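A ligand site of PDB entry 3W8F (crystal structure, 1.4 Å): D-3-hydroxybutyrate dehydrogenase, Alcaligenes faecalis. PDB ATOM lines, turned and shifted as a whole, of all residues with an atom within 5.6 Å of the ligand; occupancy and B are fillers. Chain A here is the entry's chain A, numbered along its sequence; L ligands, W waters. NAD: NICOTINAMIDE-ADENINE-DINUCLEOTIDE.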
ATOM      1  N   THR A  10     -14.825   4.355   2.052  1.00  0.00           N
ATOM      2  CA  THR A  10     -14.972   3.341   3.080  1.00  0.00           C
ATOM      3  C   THR A  10     -13.612   3.019   3.677  1.00  0.00           C
ATOM      4  O   THR A  10     -12.548   3.153   2.985  1.00  0.00           O
ATOM      5  CB  THR A  10     -15.632   2.086   2.533  1.00  0.00           C
ATOM      6  OG1 THR A  10     -14.733   1.375   1.610  1.00  0.00           O
ATOM      7  CG2 THR A  10     -16.903   2.368   1.761  1.00  0.00           C
ATOM      8  N   GLY A  11     -13.581   2.585   4.941  1.00  0.00           N
ATOM      9  CA  GLY A  11     -12.292   2.216   5.547  1.00  0.00           C
ATOM     10  C   GLY A  11     -11.281   3.387   5.488  1.00  0.00           C
ATOM     11  O   GLY A  11     -10.095   3.213   5.167  1.00  0.00           O
ATOM     12  N   SER A  12     -11.742   4.571   5.881  1.00  0.00           N
ATOM     13  CA  SER A  12     -10.924   5.820   5.778  1.00  0.00           C
ATOM     14  C   SER A  12     -10.502   6.309   7.175  1.00  0.00           C
ATOM     15  O   SER A  12     -10.043   7.431   7.272  1.00  0.00           O
ATOM     16  CB  SER A  12     -11.656   6.860   4.990  1.00  0.00           C
ATOM     17  OG  SER A  12     -13.051   6.946   5.420  1.00  0.00           O
ATOM     18  N   THR A  13     -10.506   5.431   8.159  1.00  0.00           N
ATOM     19  CA  THR A  13      -9.967   5.846   9.500  1.00  0.00           C
ATOM     20  C   THR A  13      -8.493   5.436   9.612  1.00  0.00           C
ATOM     21  O   THR A  13      -7.881   5.674  10.688  1.00  0.00           O
ATOM     22  CB  THR A  13     -10.788   5.165  10.610  1.00  0.00           C
ATOM     23  OG1 THR A  13     -10.825   3.709  10.384  1.00  0.00           O
ATOM     24  CG2 THR A  13     -12.196   5.708  10.626  1.00  0.00           C
ATOM     25  N   SER A  14      -7.860   4.884   8.621  1.00  0.00           N
ATOM     26  CA  SER A  14      -6.448   4.438   8.674  1.00  0.00           C
ATOM     27  C   SER A  14      -5.979   4.352   7.268  1.00  0.00           C
ATOM     28  O   SER A  14      -6.791   4.222   6.309  1.00  0.00           O
ATOM     29  CB  SER A  14      -6.394   2.926   9.192  1.00  0.00           C
ATOM     30  OG  SER A  14      -5.057   2.310   9.308  1.00  0.00           O
ATOM     31  N   GLY A  15      -4.671   4.324   7.112  1.00  0.00           N
ATOM     32  CA  GLY A  15      -4.057   3.789   5.925  1.00  0.00           C
ATOM     33  C   GLY A  15      -4.425   4.571   4.679  1.00  0.00           C
ATOM     34  O   GLY A  15      -4.493   5.833   4.623  1.00  0.00           O
ATOM     35  N   ILE A  16      -4.577   3.811   3.599  1.00  0.00           N
ATOM     36  CA  ILE A  16      -4.826   4.398   2.344  1.00  0.00           C
ATOM     37  C   ILE A  16      -6.118   5.209   2.317  1.00  0.00           C
ATOM     38  O   ILE A  16      -6.151   6.291   1.687  1.00  0.00           O
ATOM     39  CB  ILE A  16      -4.872   3.282   1.333  1.00  0.00           C
ATOM     40  CG1 ILE A  16      -3.488   2.613   1.158  1.00  0.00           C
ATOM     41  CG2 ILE A  16      -5.413   3.719  -0.042  1.00  0.00           C
ATOM     42  CD1 ILE A  16      -3.521   1.253   0.395  1.00  0.00           C
ATOM     43  N   GLY A  17      -7.184   4.673   2.924  1.00  0.00           N
ATOM     44  CA  GLY A  17      -8.454   5.398   2.892  1.00  0.00           C
ATOM     45  C   GLY A  17      -8.418   6.740   3.587  1.00  0.00           C
ATOM     46  O   GLY A  17      -9.045   7.684   3.122  1.00  0.00           O
ATOM     47  N   ASN A  34     -15.335   6.482   7.361  1.00  0.00           N
ATOM     48  CA  ASN A  34     -15.951   5.245   7.843  1.00  0.00           C
ATOM     49  C   ASN A  34     -14.814   4.349   8.288  1.00  0.00           C
ATOM     50  O   ASN A  34     -13.684   4.487   7.796  1.00  0.00           O
ATOM     51  CB  ASN A  34     -16.735   4.641   6.607  1.00  0.00           C
ATOM     52  CG  ASN A  34     -16.982   3.181   6.776  1.00  0.00           C
ATOM     53  OD1 ASN A  34     -16.220   2.330   6.256  1.00  0.00           O
ATOM     54  ND2 ASN A  34     -17.986   2.802   7.476  1.00  0.00           N
ATOM     55  N   GLY A  35     -15.075   3.424   9.208  1.00  0.00           N
ATOM     56  CA  GLY A  35     -14.047   2.470   9.628  1.00  0.00           C
ATOM     57  C   GLY A  35     -13.998   2.404  11.125  1.00  0.00           C
ATOM     58  O   GLY A  35     -14.672   3.131  11.827  1.00  0.00           O
ATOM     59  N   PHE A  36     -13.136   1.536  11.551  1.00  0.00           N
ATOM     60  CA  PHE A  36     -12.982   1.285  12.978  1.00  0.00           C
ATOM     61  C   PHE A  36     -11.855   2.140  13.533  1.00  0.00           C
ATOM     62  O   PHE A  36     -11.005   2.654  12.849  1.00  0.00           O
ATOM     63  CB  PHE A  36     -12.748  -0.220  13.223  1.00  0.00           C
ATOM     64  CG  PHE A  36     -13.825  -1.089  12.717  1.00  0.00           C
ATOM     65  CD1 PHE A  36     -15.140  -0.675  12.801  1.00  0.00           C
ATOM     66  CD2 PHE A  36     -13.517  -2.256  12.020  1.00  0.00           C
ATOM     67  CE1 PHE A  36     -16.193  -1.522  12.269  1.00  0.00           C
ATOM     68  CE2 PHE A  36     -14.424  -3.110  11.591  1.00  0.00           C
ATOM     69  CZ  PHE A  36     -15.816  -2.757  11.688  1.00  0.00           C
ATOM     70  N   GLY A  37     -11.812   2.269  14.855  1.00  0.00           N
ATOM     71  CA  GLY A  37     -10.644   2.956  15.463  1.00  0.00           C
ATOM     72  C   GLY A  37     -11.101   3.554  16.794  1.00  0.00           C
ATOM     73  O   GLY A  37     -12.261   3.429  17.187  1.00  0.00           O
ATOM     74  N   ALA A  62     -20.071   1.897  10.172  1.00  0.00           N
ATOM     75  CA  ALA A  62     -20.810   0.761   9.619  1.00  0.00           C
ATOM     76  C   ALA A  62     -19.824  -0.334   9.401  1.00  0.00           C
ATOM     77  O   ALA A  62     -18.703  -0.096   8.888  1.00  0.00           O
ATOM     78  CB  ALA A  62     -21.398   1.102   8.246  1.00  0.00           C
ATOM     79  N   ASP A  63     -20.131  -1.569   9.844  1.00  0.00           N
ATOM     80  CA  ASP A  63     -19.327  -2.727   9.539  1.00  0.00           C
ATOM     81  C   ASP A  63     -19.794  -3.237   8.219  1.00  0.00           C
ATOM     82  O   ASP A  63     -20.887  -3.784   8.038  1.00  0.00           O
ATOM     83  CB  ASP A  63     -19.537  -3.765  10.681  1.00  0.00           C
ATOM     84  CG  ASP A  63     -18.807  -5.047  10.427  1.00  0.00           C
ATOM     85  OD1 ASP A  63     -18.349  -5.331   9.314  1.00  0.00           O
ATOM     86  OD2 ASP A  63     -18.727  -5.892  11.370  1.00  0.00           O
ATOM     87  N   LEU A  64     -18.946  -3.041   7.223  1.00  0.00           N
ATOM     88  CA  LEU A  64     -19.370  -3.304   5.832  1.00  0.00           C
ATOM     89  C   LEU A  64     -19.255  -4.775   5.449  1.00  0.00           C
ATOM     90  O   LEU A  64     -19.552  -5.112   4.273  1.00  0.00           O
ATOM     91  CB  LEU A  64     -18.519  -2.440   4.888  1.00  0.00           C
ATOM     92  CG  LEU A  64     -18.595  -0.977   5.195  1.00  0.00           C
ATOM     93  CD1 LEU A  64     -17.613  -0.251   4.241  1.00  0.00           C
ATOM     94  CD2 LEU A  64     -19.996  -0.395   5.070  1.00  0.00           C
ATOM     95  N   SER A  65     -18.974  -5.677   6.407  1.00  0.00           N
ATOM     96  CA  SER A  65     -19.129  -7.056   6.120  1.00  0.00           C
ATOM     97  C   SER A  65     -20.573  -7.525   6.056  1.00  0.00           C
ATOM     98  O   SER A  65     -20.811  -8.648   5.690  1.00  0.00           O
ATOM     99  CB  SER A  65     -18.376  -7.871   7.156  1.00  0.00           C
ATOM    100  OG  SER A  65     -18.955  -7.785   8.434  1.00  0.00           O
ATOM    101  N   ASN A  90     -12.804   1.093  -0.414  1.00  0.00           N
ATOM    102  CA  ASN A  90     -11.430   0.903   0.046  1.00  0.00           C
ATOM    103  C   ASN A  90     -11.315  -0.057   1.196  1.00  0.00           C
ATOM    104  O   ASN A  90     -10.269  -0.752   1.306  1.00  0.00           O
ATOM    105  CB  ASN A  90     -10.823   2.268   0.408  1.00  0.00           C
ATOM    106  CG  ASN A  90      -9.566   2.148   1.174  1.00  0.00           C
ATOM    107  OD1 ASN A  90      -8.467   1.941   0.602  1.00  0.00           O
ATOM    108  ND2 ASN A  90      -9.691   2.222   2.489  1.00  0.00           N
ATOM    109  N   ALA A  91     -12.280  -0.185   2.103  1.00  0.00           N
ATOM    110  CA  ALA A  91     -12.067  -0.999   3.307  1.00  0.00           C
ATOM    111  C   ALA A  91     -11.641  -2.417   2.966  1.00  0.00           C
ATOM    112  O   ALA A  91     -12.209  -3.033   2.036  1.00  0.00           O
ATOM    113  CB  ALA A  91     -13.435  -1.036   4.107  1.00  0.00           C
ATOM    114  N   GLY A  92     -10.695  -2.999   3.657  1.00  0.00           N
ATOM    115  CA  GLY A  92     -10.275  -4.382   3.322  1.00  0.00           C
ATOM    116  C   GLY A  92      -9.460  -4.885   4.506  1.00  0.00           C
ATOM    117  O   GLY A  92      -8.889  -4.108   5.300  1.00  0.00           O
ATOM    118  N   ILE A  93      -9.393  -6.226   4.554  1.00  0.00           N
ATOM    119  CA  ILE A  93      -8.574  -6.962   5.574  1.00  0.00           C
ATOM    120  C   ILE A  93      -7.704  -8.001   4.881  1.00  0.00           C
ATOM    121  O   ILE A  93      -7.931  -8.342   3.695  1.00  0.00           O
ATOM    122  CB  ILE A  93      -9.458  -7.586   6.688  1.00  0.00           C
ATOM    123  CG1 ILE A  93     -10.516  -8.454   6.014  1.00  0.00           C
ATOM    124  CG2 ILE A  93     -10.076  -6.472   7.554  1.00  0.00           C
ATOM    125  CD1 ILE A  93     -11.228  -9.299   7.077  1.00  0.00           C
ATOM    126  N   LEU A 113     -15.931  -8.558   3.124  1.00  0.00           N
ATOM    127  CA  LEU A 113     -15.503  -7.146   3.130  1.00  0.00           C
ATOM    128  C   LEU A 113     -14.846  -6.744   1.838  1.00  0.00           C
ATOM    129  O   LEU A 113     -15.187  -5.719   1.231  1.00  0.00           O
ATOM    130  CB  LEU A 113     -14.554  -6.881   4.315  1.00  0.00           C
ATOM    131  CG  LEU A 113     -14.151  -5.409   4.370  1.00  0.00           C
ATOM    132  CD1 LEU A 113     -15.397  -4.517   4.638  1.00  0.00           C
ATOM    133  CD2 LEU A 113     -13.146  -5.326   5.526  1.00  0.00           C
ATOM    134  N   ASN A 114     -13.879  -7.566   1.400  1.00  0.00           N
ATOM    135  CA  ASN A 114     -13.050  -7.132   0.282  1.00  0.00           C
ATOM    136  C   ASN A 114     -13.759  -7.313  -1.054  1.00  0.00           C
ATOM    137  O   ASN A 114     -13.292  -6.684  -2.019  1.00  0.00           O
ATOM    138  CB  ASN A 114     -11.738  -7.911   0.243  1.00  0.00           C
ATOM    139  CG  ASN A 114     -10.826  -7.702   1.449  1.00  0.00           C
ATOM    140  OD1 ASN A 114     -11.245  -7.280   2.513  1.00  0.00           O
ATOM    141  ND2 ASN A 114      -9.533  -7.986   1.265  1.00  0.00           N
ATOM    142  N   ILE A 140     -10.540   0.000  -4.676  1.00  0.00           N
ATOM    143  CA  ILE A 140      -9.185  -0.248  -4.326  1.00  0.00           C
ATOM    144  C   ILE A 140      -8.966  -1.740  -4.342  1.00  0.00           C
ATOM    145  O   ILE A 140      -9.409  -2.480  -3.427  1.00  0.00           O
ATOM    146  CB  ILE A 140      -8.789   0.328  -2.953  1.00  0.00           C
ATOM    147  CG1 ILE A 140      -9.180   1.820  -2.828  1.00  0.00           C
ATOM    148  CG2 ILE A 140      -7.226   0.134  -2.697  1.00  0.00           C
ATOM    149  CD1 ILE A 140      -8.654   2.712  -3.977  1.00  0.00           C
ATOM    150  N   ALA A 141      -8.344  -2.219  -5.441  1.00  0.00           N
ATOM    151  CA  ALA A 141      -8.008  -3.604  -5.581  1.00  0.00           C
ATOM    152  C   ALA A 141      -6.629  -3.812  -5.109  1.00  0.00           C
ATOM    153  O   ALA A 141      -6.341  -3.507  -3.896  1.00  0.00           O
ATOM    154  CB  ALA A 141      -8.274  -4.126  -6.992  1.00  0.00           C
ATOM    155  N   SER A 142      -5.686  -4.297  -5.922  1.00  0.00           N
ATOM    156  CA  SER A 142      -4.291  -4.638  -5.472  1.00  0.00           C
ATOM    157  C   SER A 142      -3.619  -5.189  -6.682  1.00  0.00           C
ATOM    158  O   SER A 142      -4.303  -5.620  -7.644  1.00  0.00           O
ATOM    159  CB  SER A 142      -4.411  -5.770  -4.441  1.00  0.00           C
ATOM    160  OG  SER A 142      -3.098  -6.203  -4.110  1.00  0.00           O
ATOM    161  N   ALA A 143      -2.305  -5.215  -6.714  1.00  0.00           N
ATOM    162  CA  ALA A 143      -1.646  -6.110  -7.658  1.00  0.00           C
ATOM    163  C   ALA A 143      -2.125  -7.524  -7.548  1.00  0.00           C
ATOM    164  O   ALA A 143      -2.131  -8.243  -8.537  1.00  0.00           O
ATOM    165  CB  ALA A 143      -0.111  -6.035  -7.443  1.00  0.00           C
ATOM    166  N   TYR A 155      -7.676 -13.394  -0.190  1.00  0.00           N
ATOM    167  CA  TYR A 155      -7.484 -12.029  -0.599  1.00  0.00           C
ATOM    168  C   TYR A 155      -7.241 -11.887  -2.141  1.00  0.00           C
ATOM    169  O   TYR A 155      -7.828 -11.017  -2.739  1.00  0.00           O
ATOM    170  CB  TYR A 155      -6.220 -11.543   0.125  1.00  0.00           C
ATOM    171  CG  TYR A 155      -5.841 -10.067  -0.050  1.00  0.00           C
ATOM    172  CD1 TYR A 155      -6.374  -9.135   0.809  1.00  0.00           C
ATOM    173  CD2 TYR A 155      -4.949  -9.666  -1.046  1.00  0.00           C
ATOM    174  CE1 TYR A 155      -5.979  -7.788   0.757  1.00  0.00           C
ATOM    175  CE2 TYR A 155      -4.604  -8.329  -1.142  1.00  0.00           C
ATOM    176  CZ  TYR A 155      -5.083  -7.428  -0.221  1.00  0.00           C
ATOM    177  OH  TYR A 155      -4.705  -6.122  -0.285  1.00  0.00           O
ATOM    178  N   LYS A 159      -9.724  -9.866  -4.535  1.00  0.00           N
ATOM    179  CA  LYS A 159      -9.229  -8.738  -5.315  1.00  0.00           C
ATOM    180  C   LYS A 159      -9.370  -8.987  -6.815  1.00  0.00           C
ATOM    181  O   LYS A 159      -9.707  -8.059  -7.549  1.00  0.00           O
ATOM    182  CB  LYS A 159      -7.748  -8.385  -4.964  1.00  0.00           C
ATOM    183  CG  LYS A 159      -7.571  -7.929  -3.525  1.00  0.00           C
ATOM    184  CD  LYS A 159      -8.322  -6.581  -3.297  1.00  0.00           C
ATOM    185  CE  LYS A 159      -7.838  -5.939  -1.952  1.00  0.00           C
ATOM    186  NZ  LYS A 159      -8.606  -4.690  -1.765  1.00  0.00           N
ATOM    187  N   CYS A 184      -4.860  -0.407  -8.307  1.00  0.00           N
ATOM    188  CA  CYS A 184      -4.217  -1.682  -7.944  1.00  0.00           C
ATOM    189  C   CYS A 184      -2.874  -1.332  -7.364  1.00  0.00           C
ATOM    190  O   CYS A 184      -1.847  -1.341  -8.072  1.00  0.00           O
ATOM    191  CB  CYS A 184      -4.081  -2.589  -9.185  1.00  0.00           C
ATOM    192  SG  CYS A 184      -5.672  -3.188  -9.733  1.00  0.00           S
ATOM    193  N   PRO A 185      -2.750  -1.023  -6.086  1.00  0.00           N
ATOM    194  CA  PRO A 185      -1.449  -0.726  -5.501  1.00  0.00           C
ATOM    195  C   PRO A 185      -0.631  -1.953  -5.261  1.00  0.00           C
ATOM    196  O   PRO A 185      -1.140  -3.040  -5.033  1.00  0.00           O
ATOM    197  CB  PRO A 185      -1.778  -0.111  -4.075  1.00  0.00           C
ATOM    198  CG  PRO A 185      -3.297   0.163  -4.117  1.00  0.00           C
ATOM    199  CD  PRO A 185      -3.870  -0.908  -5.096  1.00  0.00           C
ATOM    200  N   GLY A 186       0.695  -1.754  -5.366  1.00  0.00           N
ATOM    201  CA  GLY A 186       1.657  -2.659  -4.750  1.00  0.00           C
ATOM    202  C   GLY A 186       1.777  -2.341  -3.263  1.00  0.00           C
ATOM    203  O   GLY A 186       0.807  -1.810  -2.617  1.00  0.00           O
ATOM    204  N   TRP A 187       2.892  -2.727  -2.645  1.00  0.00           N
ATOM    205  CA  TRP A 187       3.004  -2.571  -1.181  1.00  0.00           C
ATOM    206  C   TRP A 187       2.945  -1.111  -0.755  1.00  0.00           C
ATOM    207  O   TRP A 187       3.657  -0.260  -1.329  1.00  0.00           O
ATOM    208  CB  TRP A 187       4.384  -3.065  -0.707  1.00  0.00           C
ATOM    209  CG  TRP A 187       4.639  -4.511  -0.864  1.00  0.00           C
ATOM    210  CD1 TRP A 187       5.735  -5.038  -1.498  1.00  0.00           C
ATOM    211  CD2 TRP A 187       3.956  -5.624  -0.272  1.00  0.00           C
ATOM    212  NE1 TRP A 187       5.791  -6.417  -1.338  1.00  0.00           N
ATOM    213  CE2 TRP A 187       4.719  -6.794  -0.561  1.00  0.00           C
ATOM    214  CE3 TRP A 187       2.790  -5.753   0.510  1.00  0.00           C
ATOM    215  CZ2 TRP A 187       4.360  -8.086  -0.149  1.00  0.00           C
ATOM    216  CZ3 TRP A 187       2.477  -7.051   0.918  1.00  0.00           C
ATOM    217  CH2 TRP A 187       3.270  -8.176   0.626  1.00  0.00           C
ATOM    218  N   VAL A 188       2.173  -0.818   0.276  1.00  0.00           N
ATOM    219  CA  VAL A 188       2.006   0.468   0.963  1.00  0.00           C
ATOM    220  C   VAL A 188       2.174   0.162   2.426  1.00  0.00           C
ATOM    221  O   VAL A 188       1.596  -0.768   2.968  1.00  0.00           O
ATOM    222  CB  VAL A 188       0.588   1.026   0.711  1.00  0.00           C
ATOM    223  CG1 VAL A 188       0.416   2.415   1.290  1.00  0.00           C
ATOM    224  CG2 VAL A 188       0.243   1.059  -0.798  1.00  0.00           C
ATOM    225  N   ARG A 189       3.034   0.946   3.113  1.00  0.00           N
ATOM    226  CA  ARG A 189       3.333   0.632   4.496  1.00  0.00           C
ATOM    227  C   ARG A 189       2.312   1.114   5.482  1.00  0.00           C
ATOM    228  O   ARG A 189       2.487   2.085   6.163  1.00  0.00           O
ATOM    229  CB  ARG A 189       4.743   1.099   4.807  1.00  0.00           C
ATOM    230  CG  ARG A 189       5.280   0.379   6.036  1.00  0.00           C
ATOM    231  CD  ARG A 189       6.714   0.697   6.248  1.00  0.00           C
ATOM    232  NE  ARG A 189       7.214  -0.101   7.387  1.00  0.00           N
ATOM    233  CZ  ARG A 189       8.498  -0.156   7.705  1.00  0.00           C
ATOM    234  NH1 ARG A 189       9.420   0.540   7.049  1.00  0.00           N
ATOM    235  NH2 ARG A 189       8.806  -0.855   8.780  1.00  0.00           N
ATOM    236  N   THR A 190       1.223   0.424   5.529  1.00  0.00           N
ATOM    237  CA  THR A 190       0.095   0.618   6.469  1.00  0.00           C
ATOM    238  C   THR A 190       0.103  -0.545   7.477  1.00  0.00           C
ATOM    239  O   THR A 190       0.878  -1.475   7.382  1.00  0.00           O
ATOM    240  CB  THR A 190      -1.259   0.513   5.721  1.00  0.00           C
ATOM    241  OG1 THR A 190      -1.368  -0.836   5.347  1.00  0.00           O
ATOM    242  CG2 THR A 190      -1.278   1.374   4.477  1.00  0.00           C
ATOM    243  N   PRO A 191      -0.805  -0.476   8.496  1.00  0.00           N
ATOM    244  CA  PRO A 191      -0.852  -1.603   9.456  1.00  0.00           C
ATOM    245  C   PRO A 191      -1.094  -2.952   8.842  1.00  0.00           C
ATOM    246  O   PRO A 191      -0.552  -3.962   9.365  1.00  0.00           O
ATOM    247  CB  PRO A 191      -1.943  -1.185  10.434  1.00  0.00           C
ATOM    248  CG  PRO A 191      -1.993   0.345  10.307  1.00  0.00           C
ATOM    249  CD  PRO A 191      -1.637   0.662   8.878  1.00  0.00           C
ATOM    250  N   LEU A 192      -1.780  -2.991   7.681  1.00  0.00           N
ATOM    251  CA  LEU A 192      -2.066  -4.265   7.038  1.00  0.00           C
ATOM    252  C   LEU A 192      -0.752  -4.890   6.542  1.00  0.00           C
ATOM    253  O   LEU A 192      -0.659  -6.130   6.572  1.00  0.00           O
ATOM    254  CB  LEU A 192      -3.017  -3.937   5.879  1.00  0.00           C
ATOM    255  CG  LEU A 192      -3.524  -5.145   5.048  1.00  0.00           C
ATOM    256  CD1 LEU A 192      -4.943  -4.864   4.577  1.00  0.00           C
ATOM    257  CD2 LEU A 192      -2.550  -5.474   3.881  1.00  0.00           C
ATOM    258  N   VAL A 193       0.222  -4.094   6.140  1.00  0.00           N
ATOM    259  CA  VAL A 193       1.530  -4.567   5.706  1.00  0.00           C
ATOM    260  C   VAL A 193       2.491  -4.666   6.856  1.00  0.00           C
ATOM    261  O   VAL A 193       3.315  -5.575   6.845  1.00  0.00           O
ATOM    262  CB  VAL A 193       2.008  -3.645   4.605  1.00  0.00           C
ATOM    263  CG1 VAL A 193       3.506  -3.817   4.276  1.00  0.00           C
ATOM    264  CG2 VAL A 193       1.211  -4.025   3.354  1.00  0.00           C
HETATM  265  PA  NAD L   1      -5.600  -0.523   6.942  1.00  0.00           P
HETATM  266  O1A NAD L   1      -5.720  -1.663   7.734  1.00  0.00           O
HETATM  267  O2A NAD L   1      -4.684   0.571   7.272  1.00  0.00           O
HETATM  268  O5B NAD L   1      -6.984   0.192   6.761  1.00  0.00           O
HETATM  269  C5B NAD L   1      -8.210  -0.644   6.591  1.00  0.00           C
HETATM  270  C4B NAD L   1      -9.349   0.364   6.833  1.00  0.00           C
HETATM  271  O4B NAD L   1     -10.548  -0.494   6.693  1.00  0.00           O
HETATM  272  C3B NAD L   1      -9.420   0.877   8.284  1.00  0.00           C
HETATM  273  O3B NAD L   1     -10.031   2.183   8.207  1.00  0.00           O
HETATM  274  C2B NAD L   1     -10.302  -0.139   8.952  1.00  0.00           C
HETATM  275  O2B NAD L   1     -10.927   0.389  10.140  1.00  0.00           O
HETATM  276  C1B NAD L   1     -11.341  -0.360   7.875  1.00  0.00           C
HETATM  277  N9A NAD L   1     -12.098  -1.517   8.067  1.00  0.00           N
HETATM  278  C8A NAD L   1     -11.678  -2.822   8.384  1.00  0.00           C
HETATM  279  N7A NAD L   1     -12.710  -3.664   8.503  1.00  0.00           N
HETATM  280  C5A NAD L   1     -13.863  -2.931   8.224  1.00  0.00           C
HETATM  281  C6A NAD L   1     -15.226  -3.270   8.196  1.00  0.00           C
HETATM  282  N6A NAD L   1     -15.660  -4.536   8.489  1.00  0.00           N
HETATM  283  N1A NAD L   1     -16.038  -2.280   7.857  1.00  0.00           N
HETATM  284  C2A NAD L   1     -15.624  -1.009   7.629  1.00  0.00           C
HETATM  285  N3A NAD L   1     -14.342  -0.650   7.662  1.00  0.00           N
HETATM  286  C4A NAD L   1     -13.476  -1.645   7.939  1.00  0.00           C
HETATM  287  O3  NAD L   1      -5.244  -1.063   5.453  1.00  0.00           O
HETATM  288  PN  NAD L   1      -4.839  -0.419   4.086  1.00  0.00           P
HETATM  289  O1N NAD L   1      -3.546  -1.024   3.788  1.00  0.00           O
HETATM  290  O2N NAD L   1      -4.967   1.003   4.116  1.00  0.00           O
HETATM  291  O5D NAD L   1      -5.939  -1.053   3.152  1.00  0.00           O
HETATM  292  C5D NAD L   1      -6.939  -0.318   2.433  1.00  0.00           C
HETATM  293  C4D NAD L   1      -7.226  -1.052   1.157  1.00  0.00           C
HETATM  294  O4D NAD L   1      -6.014  -1.053   0.339  1.00  0.00           O
HETATM  295  C3D NAD L   1      -7.644  -2.492   1.416  1.00  0.00           C
HETATM  296  O3D NAD L   1      -8.680  -2.841   0.453  1.00  0.00           O
HETATM  297  C2D NAD L   1      -6.399  -3.248   0.973  1.00  0.00           C
HETATM  298  O2D NAD L   1      -6.715  -4.540   0.472  1.00  0.00           O
HETATM  299  C1D NAD L   1      -5.897  -2.382  -0.163  1.00  0.00           C
HETATM  300  N1N NAD L   1      -4.481  -2.540  -0.463  1.00  0.00           N
HETATM  301  C2N NAD L   1      -3.481  -2.338   0.470  1.00  0.00           C
HETATM  302  C3N NAD L   1      -2.173  -2.503   0.145  1.00  0.00           C
HETATM  303  C7N NAD L   1      -1.068  -2.313   1.043  1.00  0.00           C
HETATM  304  O7N NAD L   1       0.100  -2.677   0.669  1.00  0.00           O
HETATM  305  N7N NAD L   1      -1.324  -1.762   2.248  1.00  0.00           N
HETATM  306  C4N NAD L   1      -1.845  -2.893  -1.194  1.00  0.00           C
HETATM  307  C5N NAD L   1      -2.861  -3.085  -2.139  1.00  0.00           C
HETATM  308  C6N NAD L   1      -4.181  -2.883  -1.787  1.00  0.00           C
HETATM  309  O   HOH W   1      -8.689  -3.416   9.627  1.00  0.00           O
HETATM  310  O   HOH W   2      -7.188  -4.084   7.466  1.00  0.00           O
HETATM  311  O   HOH W   3      -7.393   2.233   4.399  1.00  0.00           O
HETATM  312  O   HOH W   4     -14.496  -7.309   9.041  1.00  0.00           O
HETATM  313  O   HOH W   5      -6.737  -1.082  10.502  1.00  0.00           O
HETATM  314  O   HOH W   6     -12.336  -5.874  10.329  1.00  0.00           O
HETATM  315  O   HOH W   7      -8.995   0.059  11.964  1.00  0.00           O
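The side-chain hydroxyl (OH) of Tyr 155 is in hydrogen-bond range of an oxygen (O2D) of the ligand, 2.7 Å away.
O7N of the ligand sits at hydrogen-bond distance from N of Val 188 (2.8 Å).
The side-chain carboxylate of Asp 63 sits at hydrogen-bond distance from a nitrogen (N6A) of the ligand.
The side-chain amino group (NZ) of Lys 159 lies within hydrogen-bond range of an oxygen (O3D) of the ligand (2.9 Å).
An oxygen (O3B) of the ligand is in hydrogen-bond range of the backbone carbonyl oxygen (O) of Gly 11 (3.2 Å).
O3B of the ligand is in hydrogen-bond range of OG1 of Thr 13 (2.8 Å).
The backbone NH of Ile 16 is in hydrogen-bond range of an oxygen (O2N) of the ligand.
The side-chain hydroxyl (OG) of Ser 14 lies within hydrogen-bond range of an oxygen (O2A) of the ligand (2.7 Å).
A nitrogen (N1A) of the ligand sits at hydrogen-bond distance from the backbone NH (N) of Leu 64 (3.1 Å).
N of Ser 14 lies within hydrogen-bond range of O3B of the ligand (3.5 Å).
O3B of the ligand sits at hydrogen-bond distance from N of Thr 13, at 3.3 Å.
A nitrogen (N7N) of the ligand is in hydrogen-bond range of the backbone carbonyl oxygen (O) of Val 188, at 3.2 Å.
O of Asn 90 lies within hydrogen-bond range of O3D of the ligand, 2.8 Å away.
OG1 of Thr 190 sits at hydrogen-bond distance from O1N of the ligand (2.7 Å).
An oxygen (O2B) of the ligand lies within hydrogen-bond range of the backbone NH (N) of Phe 36, at 2.9 Å.
The backbone carbonyl oxygen of Gly 186 lies close to an oxygen (O7N) of the ligand, 3.5 Å away.
Residues that only touch the ligand: Ser 12 (3.7 Å), Gly 15 (3.4 Å), Asn 34 (3.7 Å), Gly 35 (3.7 Å), Ala 62 (3.4 Å), Ala 91 (3.7 Å), Gly 92 (3.6 Å), Ile 93 (3.97 Å), Leu 113 (3.4 Å), Ile 140 (3.5 Å), Ala 141 (3.1 Å), Ser 142 (3.7 Å), Pro 185 (3.4 Å), Trp 187 (3.4 Å), Pro 191 (3.4 Å), Leu 192 (3.6 Å) and Val 193 (3.2 Å).
Hydrophobic or aromatic side chains that line the ligand: Ile 16, Phe 36, Leu 64, Ala 91, Ile 93, Leu 113, Ile 140, Tyr 155, Pro 185, Val 188, Pro 191, Leu 192 and Val 193.
Within 4 Å of the ligand: Gly 11, Ser 12, Thr 13, Ser 14, Gly 15, Ile 16, Asn 34, Gly 35, Phe 36, Ala 62, Asp 63, Leu 64, Asn 90, Ala 91, Gly 92, Ile 93, Leu 113, Ile 140, Ala 141, Ser 142, Tyr 155, Lys 159, Pro 185, Gly 186, Trp 187, Val 188, Thr 190, Pro 191, Leu 192 and Val 193.
The nearest printed residue that does not touch the ligand is Ser 65 (4.1 Å).
Water W7 lies within hydrogen-bond range of an oxygen (O2B) of the ligand (2.7 Å) and the backbone carbonyl oxygen (O) of Phe 36 (3.4 Å).
Water W2 lies within hydrogen-bond range of the backbone carbonyl oxygen (O) of Gly 92 (2.8 Å) and an oxygen (O1A) of the ligand (2.8 Å).
The side-chain amino group of Lys 159 lies within hydrogen-bond range of the backbone carbonyl oxygen of Ala 141, at 3.3 Å.
The backbone carbonyl oxygen (O) of Ile 140 is in hydrogen-bond range of the side-chain amino group (NZ) of Lys 159.
OG1 of Thr 10 lies within hydrogen-bond range of N of Ala 91 (2.9 Å).
The backbone NH of Ala 143 sits at hydrogen-bond distance from the backbone carbonyl oxygen of Pro 185, at 3.0 Å.
N of Ser 12 lies within hydrogen-bond range of O of Asn 34.
ND2 of Asn 90 sits at hydrogen-bond distance from O of Gly 11.
O of Ser 142 lies close to SG of Cys 184.
O of Phe 36 sits at hydrogen-bond distance from OG1 of Thr 13, 2.7 Å away.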
